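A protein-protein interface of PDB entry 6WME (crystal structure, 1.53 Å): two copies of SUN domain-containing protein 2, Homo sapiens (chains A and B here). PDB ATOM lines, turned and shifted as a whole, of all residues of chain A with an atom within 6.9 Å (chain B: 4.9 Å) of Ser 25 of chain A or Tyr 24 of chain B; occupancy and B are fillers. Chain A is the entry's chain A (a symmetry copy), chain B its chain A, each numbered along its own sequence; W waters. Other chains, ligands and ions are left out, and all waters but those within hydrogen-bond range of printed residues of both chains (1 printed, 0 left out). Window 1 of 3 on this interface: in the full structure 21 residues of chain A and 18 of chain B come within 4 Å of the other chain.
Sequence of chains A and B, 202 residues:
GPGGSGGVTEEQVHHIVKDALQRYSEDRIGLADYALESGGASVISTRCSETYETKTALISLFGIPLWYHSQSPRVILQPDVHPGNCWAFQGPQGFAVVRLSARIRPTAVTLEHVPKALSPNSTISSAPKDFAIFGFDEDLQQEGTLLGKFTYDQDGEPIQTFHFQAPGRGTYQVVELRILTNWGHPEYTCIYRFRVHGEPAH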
ATOM      1  N   ALA A  20      19.856  -6.483  27.285  1.00  0.00           N
ATOM      2  CA  ALA A  20      19.416  -7.166  26.076  1.00  0.00           C
ATOM      3  C   ALA A  20      17.998  -6.765  25.692  1.00  0.00           C
ATOM      4  O   ALA A  20      17.697  -6.559  24.506  1.00  0.00           O
ATOM      5  CB  ALA A  20      19.501  -8.673  26.282  1.00  0.00           C
ATOM      6  N   LEU A  21      17.107  -6.650  26.678  1.00  0.00           N
ATOM      7  CA  LEU A  21      15.736  -6.247  26.376  1.00  0.00           C
ATOM      8  C   LEU A  21      15.663  -4.779  26.000  1.00  0.00           C
ATOM      9  O   LEU A  21      14.799  -4.387  25.203  1.00  0.00           O
ATOM     10  CB  LEU A  21      14.824  -6.538  27.568  1.00  0.00           C
ATOM     11  CG  LEU A  21      14.435  -8.006  27.721  1.00  0.00           C
ATOM     12  CD1 LEU A  21      13.637  -8.242  29.009  1.00  0.00           C
ATOM     13  CD2 LEU A  21      13.660  -8.478  26.514  1.00  0.00           C
ATOM     14  N   GLN A  22      16.549  -3.947  26.550  1.00  0.00           N
ATOM     15  CA  GLN A  22      16.531  -2.548  26.131  1.00  0.00           C
ATOM     16  C   GLN A  22      16.946  -2.409  24.670  1.00  0.00           C
ATOM     17  O   GLN A  22      16.285  -1.696  23.898  1.00  0.00           O
ATOM     18  CB  GLN A  22      17.419  -1.697  27.034  1.00  0.00           C
ATOM     19  CG  GLN A  22      17.317  -0.217  26.686  1.00  0.00           C
ATOM     20  CD  GLN A  22      15.866   0.292  26.676  1.00  0.00           C
ATOM     21  OE1 GLN A  22      14.978  -0.270  27.326  1.00  0.00           O
ATOM     22  NE2 GLN A  22      15.622   1.337  25.897  1.00  0.00           N
ATOM     23  N   ARG A  23      18.007  -3.113  24.257  1.00  0.00           N
ATOM     24  CA  ARG A  23      18.379  -3.126  22.842  1.00  0.00           C
ATOM     25  C   ARG A  23      17.252  -3.685  21.982  1.00  0.00           C
ATOM     26  O   ARG A  23      16.979  -3.165  20.893  1.00  0.00           O
ATOM     27  CB  ARG A  23      19.655  -3.944  22.630  1.00  0.00           C
ATOM     28  CG  ARG A  23      20.100  -4.073  21.166  1.00  0.00           C
ATOM     29  CD  ARG A  23      20.382  -2.714  20.517  1.00  0.00           C
ATOM     30  NE  ARG A  23      21.419  -1.969  21.230  1.00  0.00           N
ATOM     31  CZ  ARG A  23      22.724  -2.147  21.051  1.00  0.00           C
ATOM     32  NH1 ARG A  23      23.594  -1.428  21.749  1.00  0.00           N
ATOM     33  NH2 ARG A  23      23.162  -3.045  20.178  1.00  0.00           N
ATOM     34  N   TYR A  24      16.596  -4.750  22.449  1.00  0.00           N
ATOM     35  CA  TYR A  24      15.470  -5.329  21.715  1.00  0.00           C
ATOM     36  C   TYR A  24      14.392  -4.284  21.456  1.00  0.00           C
ATOM     37  O   TYR A  24      13.871  -4.168  20.337  1.00  0.00           O
ATOM     38  CB  TYR A  24      14.882  -6.511  22.500  1.00  0.00           C
ATOM     39  CG  TYR A  24      13.902  -7.363  21.698  1.00  0.00           C
ATOM     40  CD1 TYR A  24      12.555  -7.038  21.628  1.00  0.00           C
ATOM     41  CD2 TYR A  24      14.342  -8.482  20.995  1.00  0.00           C
ATOM     42  CE1 TYR A  24      11.667  -7.818  20.882  1.00  0.00           C
ATOM     43  CE2 TYR A  24      13.468  -9.259  20.251  1.00  0.00           C
ATOM     44  CZ  TYR A  24      12.131  -8.918  20.191  1.00  0.00           C
ATOM     45  OH  TYR A  24      11.245  -9.686  19.451  1.00  0.00           O
ATOM     46  N   SER A  25      14.067  -3.496  22.485  1.00  0.00           N
ATOM     47  CA  SER A  25      13.005  -2.497  22.394  1.00  0.00           C
ATOM     48  C   SER A  25      13.371  -1.317  21.502  1.00  0.00           C
ATOM     49  O   SER A  25      12.461  -0.614  21.037  1.00  0.00           O
ATOM     50  CB  SER A  25      12.657  -1.995  23.801  1.00  0.00           C
ATOM     51  OG  SER A  25      13.647  -1.091  24.284  1.00  0.00           O
ATOM     52  N   GLU A  26      14.664  -1.073  21.270  1.00  0.00           N
ATOM     53  CA  GLU A  26      15.121   0.040  20.433  1.00  0.00           C
ATOM     54  C   GLU A  26      15.165  -0.382  18.963  1.00  0.00           C
ATOM     55  O   GLU A  26      16.210  -0.352  18.313  1.00  0.00           O
ATOM     56  CB  GLU A  26      16.497   0.527  20.893  1.00  0.00           C
ATOM     57  CG  GLU A  26      16.551   1.095  22.309  1.00  0.00           C
ATOM     58  CD  GLU A  26      17.977   1.357  22.787  1.00  0.00           C
ATOM     59  OE1 GLU A  26      18.936   0.891  22.128  1.00  0.00           O
ATOM     60  OE2 GLU A  26      18.142   2.027  23.830  1.00  0.00           O
ATOM     61  N   ASP A  27      14.003  -0.792  18.442  1.00  0.00           N
ATOM     62  CA  ASP A  27      13.910  -1.233  17.039  1.00  0.00           C
ATOM     63  C   ASP A  27      14.927  -2.349  16.754  1.00  0.00           C
ATOM     64  O   ASP A  27      15.496  -2.426  15.666  1.00  0.00           O
ATOM     65  CB  ASP A  27      14.103  -0.030  16.093  1.00  0.00           C
ATOM     66  CG  ASP A  27      13.396  -0.177  14.738  1.00  0.00           C
ATOM     67  OD1 ASP A  27      12.593  -1.119  14.525  1.00  0.00           O
ATOM     68  OD2 ASP A  27      13.660   0.695  13.868  1.00  0.00           O
ATOM     69  N   ARG A  28      15.181  -3.193  17.772  1.00  0.00           N
ATOM     70  CA  ARG A  28      16.050  -4.378  17.748  1.00  0.00           C
ATOM     71  C   ARG A  28      17.545  -4.077  17.661  1.00  0.00           C
ATOM     72  O   ARG A  28      18.357  -4.824  18.224  1.00  0.00           O
ATOM     73  CB  ARG A  28      15.679  -5.325  16.595  1.00  0.00           C
ATOM     74  CG  ARG A  28      14.317  -5.970  16.706  1.00  0.00           C
ATOM     75  CD  ARG A  28      14.240  -6.922  17.876  1.00  0.00           C
ATOM     76  NE  ARG A  28      15.382  -7.833  17.944  1.00  0.00           N
ATOM     77  CZ  ARG A  28      15.474  -8.977  17.271  1.00  0.00           C
ATOM     78  NH1 ARG A  28      14.495  -9.362  16.458  1.00  0.00           N
ATOM     79  NH2 ARG A  28      16.558  -9.733  17.406  1.00  0.00           N
ATOM     80  N   ILE A  29      17.934  -3.021  16.950  1.00  0.00           N
ATOM     81  CA  ILE A  29      19.335  -2.776  16.639  1.00  0.00           C
ATOM     82  C   ILE A  29      19.856  -1.456  17.189  1.00  0.00           C
ATOM     83  O   ILE A  29      21.068  -1.203  17.089  1.00  0.00           O
ATOM     84  CB  ILE A  29      19.600  -2.853  15.117  1.00  0.00           C
ATOM     85  CG1 ILE A  29      18.847  -1.752  14.364  1.00  0.00           C
ATOM     86  CG2 ILE A  29      19.213  -4.214  14.581  1.00  0.00           C
ATOM     87  CD1 ILE A  29      19.167  -1.694  12.858  1.00  0.00           C
ATOM     88  N   GLY A  30      19.004  -0.596  17.745  1.00  0.00           N
ATOM     89  CA  GLY A  30      19.493   0.602  18.412  1.00  0.00           C
ATOM     90  C   GLY A  30      20.111   1.656  17.515  1.00  0.00           C
ATOM     91  O   GLY A  30      20.957   2.429  17.977  1.00  0.00           O
ATOM     92  N   ALA B  20      11.615 -12.309  32.840  1.00  0.00           N
ATOM     93  CA  ALA B  20      11.850 -11.011  32.220  1.00  0.00           C
ATOM     94  C   ALA B  20      11.066 -10.860  30.924  1.00  0.00           C
ATOM     95  O   ALA B  20      10.501  -9.792  30.645  1.00  0.00           O
ATOM     96  CB  ALA B  20      13.341 -10.834  31.959  1.00  0.00           C
ATOM     97  N   LEU B  21      11.019 -11.919  30.111  1.00  0.00           N
ATOM     98  CA  LEU B  21      10.264 -11.843  28.863  1.00  0.00           C
ATOM     99  C   LEU B  21       8.769 -11.846  29.121  1.00  0.00           C
ATOM    100  O   LEU B  21       8.006 -11.247  28.350  1.00  0.00           O
ATOM    101  CB  LEU B  21      10.647 -13.001  27.943  1.00  0.00           C
ATOM    102  CG  LEU B  21      11.985 -12.823  27.228  1.00  0.00           C
ATOM    103  CD1 LEU B  21      12.365 -14.078  26.434  1.00  0.00           C
ATOM    104  CD2 LEU B  21      11.950 -11.609  26.331  1.00  0.00           C
ATOM    105  N   GLN B  22       8.320 -12.504  30.193  1.00  0.00           N
ATOM    106  CA  GLN B  22       6.891 -12.443  30.487  1.00  0.00           C
ATOM    107  C   GLN B  22       6.473 -11.032  30.882  1.00  0.00           C
ATOM    108  O   GLN B  22       5.459 -10.517  30.383  1.00  0.00           O
ATOM    109  CB  GLN B  22       6.515 -13.449  31.573  1.00  0.00           C
ATOM    110  CG  GLN B  22       5.011 -13.484  31.806  1.00  0.00           C
ATOM    111  CD  GLN B  22       4.214 -13.724  30.514  1.00  0.00           C
ATOM    112  OE1 GLN B  22       4.718 -14.290  29.538  1.00  0.00           O
ATOM    113  NE2 GLN B  22       2.975 -13.249  30.497  1.00  0.00           N
ATOM    114  N   ARG B  23       7.259 -10.369  31.739  1.00  0.00           N
ATOM    115  CA  ARG B  23       6.987  -8.967  32.058  1.00  0.00           C
ATOM    116  C   ARG B  23       7.046  -8.097  30.809  1.00  0.00           C
ATOM    117  O   ARG B  23       6.217  -7.195  30.633  1.00  0.00           O
ATOM    118  CB  ARG B  23       7.980  -8.453  33.103  1.00  0.00           C
ATOM    119  CG  ARG B  23       7.819  -6.969  33.465  1.00  0.00           C
ATOM    120  CD  ARG B  23       6.433  -6.651  34.035  1.00  0.00           C
ATOM    121  NE  ARG B  23       6.142  -7.431  35.236  1.00  0.00           N
ATOM    122  CZ  ARG B  23       6.546  -7.103  36.460  1.00  0.00           C
ATOM    123  NH1 ARG B  23       6.238  -7.879  37.492  1.00  0.00           N
ATOM    124  NH2 ARG B  23       7.261  -6.003  36.653  1.00  0.00           N
ATOM    125  N   TYR B  24       8.028  -8.344  29.936  1.00  0.00           N
ATOM    126  CA  TYR B  24       8.139  -7.590  28.686  1.00  0.00           C
ATOM    127  C   TYR B  24       6.854  -7.690  27.874  1.00  0.00           C
ATOM    128  O   TYR B  24       6.343  -6.681  27.363  1.00  0.00           O
ATOM    129  CB  TYR B  24       9.327  -8.109  27.863  1.00  0.00           C
ATOM    130  CG  TYR B  24       9.709  -7.210  26.691  1.00  0.00           C
ATOM    131  CD1 TYR B  24       9.093  -7.339  25.453  1.00  0.00           C
ATOM    132  CD2 TYR B  24      10.677  -6.220  26.839  1.00  0.00           C
ATOM    133  CE1 TYR B  24       9.442  -6.503  24.388  1.00  0.00           C
ATOM    134  CE2 TYR B  24      11.027  -5.385  25.788  1.00  0.00           C
ATOM    135  CZ  TYR B  24      10.400  -5.526  24.566  1.00  0.00           C
ATOM    136  OH  TYR B  24      10.739  -4.701  23.505  1.00  0.00           O
ATOM    137  N   SER B  25       6.307  -8.904  27.770  1.00  0.00           N
ATOM    138  CA  SER B  25       5.112  -9.152  26.966  1.00  0.00           C
ATOM    139  C   SER B  25       3.852  -8.548  27.570  1.00  0.00           C
ATOM    140  O   SER B  25       2.872  -8.349  26.835  1.00  0.00           O
ATOM    141  CB  SER B  25       4.928 -10.663  26.783  1.00  0.00           C
ATOM    142  OG  SER B  25       4.417 -11.266  27.969  1.00  0.00           O
ATOM    143  N   GLU B  26       3.842  -8.273  28.877  1.00  0.00           N
ATOM    144  CA  GLU B  26       2.678  -7.697  29.557  1.00  0.00           C
ATOM    145  C   GLU B  26       2.704  -6.172  29.460  1.00  0.00           C
ATOM    146  O   GLU B  26       2.736  -5.461  30.465  1.00  0.00           O
ATOM    147  CB  GLU B  26       2.637  -8.142  31.019  1.00  0.00           C
ATOM    148  CG  GLU B  26       2.479  -9.643  31.244  1.00  0.00           C
ATOM    149  CD  GLU B  26       2.665 -10.047  32.704  1.00  0.00           C
ATOM    150  OE1 GLU B  26       3.141  -9.214  33.511  1.00  0.00           O
ATOM    151  OE2 GLU B  26       2.340 -11.204  33.049  1.00  0.00           O
ATOM    152  N   ASP B  27       2.705  -5.667  28.221  1.00  0.00           N
ATOM    153  CA  ASP B  27       2.738  -4.212  27.988  1.00  0.00           C
ATOM    154  C   ASP B  27       3.935  -3.575  28.711  1.00  0.00           C
ATOM    155  O   ASP B  27       3.850  -2.457  29.216  1.00  0.00           O
ATOM    156  CB  ASP B  27       1.402  -3.576  28.429  1.00  0.00           C
ATOM    157  CG  ASP B  27       1.038  -2.293  27.669  1.00  0.00           C
ATOM    158  OD1 ASP B  27       1.695  -1.925  26.664  1.00  0.00           O
ATOM    159  OD2 ASP B  27       0.049  -1.644  28.104  1.00  0.00           O
ATOM    160  N   ARG B  28       5.047  -4.330  28.791  1.00  0.00           N
ATOM    161  CA  ARG B  28       6.346  -3.942  29.361  1.00  0.00           C
ATOM    162  C   ARG B  28       6.365  -3.803  30.881  1.00  0.00           C
ATOM    163  O   ARG B  28       7.388  -4.093  31.514  1.00  0.00           O
ATOM    164  CB  ARG B  28       6.858  -2.629  28.748  1.00  0.00           C
ATOM    165  CG  ARG B  28       7.199  -2.695  27.277  1.00  0.00           C
ATOM    166  CD  ARG B  28       8.381  -3.599  27.015  1.00  0.00           C
ATOM    167  NE  ARG B  28       9.504  -3.342  27.916  1.00  0.00           N
ATOM    168  CZ  ARG B  28      10.427  -2.404  27.721  1.00  0.00           C
ATOM    169  NH1 ARG B  28      10.366  -1.610  26.658  1.00  0.00           N
ATOM    170  NH2 ARG B  28      11.409  -2.256  28.603  1.00  0.00           N
HETATM  171  O   HOH W   1      11.778   0.919  26.433  1.00  0.00           O
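O of Gln 22 of chain A is in hydrogen-bond range of OG of Ser 25 of chain A, 2.7 Å away.
Leu 21 of chain A touches its own counterpart, Leu 21 of chain B.
Leu 21 of chain A touches Tyr 24 of chain B, but with the chains exchanged Tyr 24 of chain A does not touch Leu 21 of chain B (6.6 Å).
Tyr 24 of chain B touches its own counterpart, Tyr 24 of chain A.
Ser 25 of chain A touches Arg 28 of chain B, but with the chains exchanged Arg 28 of chain A does not touch Ser 25 of chain B (12.8 Å).
Of the 6 pairs that touch across the chains among the printed residues, 2 have their exchanged pair printed and touching as well.
Leu 21 of chain A touches Ala 20 of chain B (CD1 to O, 3.9 Å).
Leu 21 of chain A touches Leu 21 of chain B (CD2 to CD2, 3.6 Å).
Leu 21 of chain A touches Tyr 24 of chain B.
OH of Tyr 24 of chain B touches CD1 of Tyr 24 of chain A, at 3.5 Å.
Ser 25 of chain A touches Tyr 24 of chain B (CB to OH, 3.3 Å).
Arg 28 of chain B touches Ser 25 of chain A.
Printed residues of chain B within 4 Å of Ser 25 of chain A: Tyr 24 (3.3 Å) and Arg 28 (3.7 Å).
Tyr 24 of chain B touches just these residues of chain A: Leu 21 (3.8 Å), Tyr 24 (3.5 Å) and Ser 25 (3.3 Å).
Of the printed residues of chain B, Leu 21 of chain A touches Ala 20, Leu 21 and Tyr 24.
Printed residues of chain A within 4 Å of Leu 21 of chain B: Leu 21.
Glu 26 of chain B touches none of the printed residues of chain A.
Ile 29 of chain A touches none of the printed residues of chain B.
The nearest residue of chain A that does not touch Tyr 24 of chain B is Gln 22 of chain A (5.8 Å).
The nearest printed residue of chain A that does not touch Leu 21 of chain B is Tyr 24 of chain A (6.6 Å).
Hydrophobic or aromatic side chains of chain B that line the printed part of chain A: Ala 20, Leu 21 and Tyr 24.
Along chain B the printed residues that touch a printed residue of chain A span positions 20 to 28.
Hydrophobic or aromatic side chains of chain A that line the printed part of chain B: Leu 21 and Tyr 24.
Among the printed residues, no Asp or Glu carboxylate lies within 4 Å of a Lys or Arg side-chain nitrogen of the other chain.
Water W1 bridges the guanidinium group (NH1) of Arg 28 of chain B (2.9 Å) and the side-chain hydroxyl (OG) of Ser 25 of chain A (3.5 Å).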
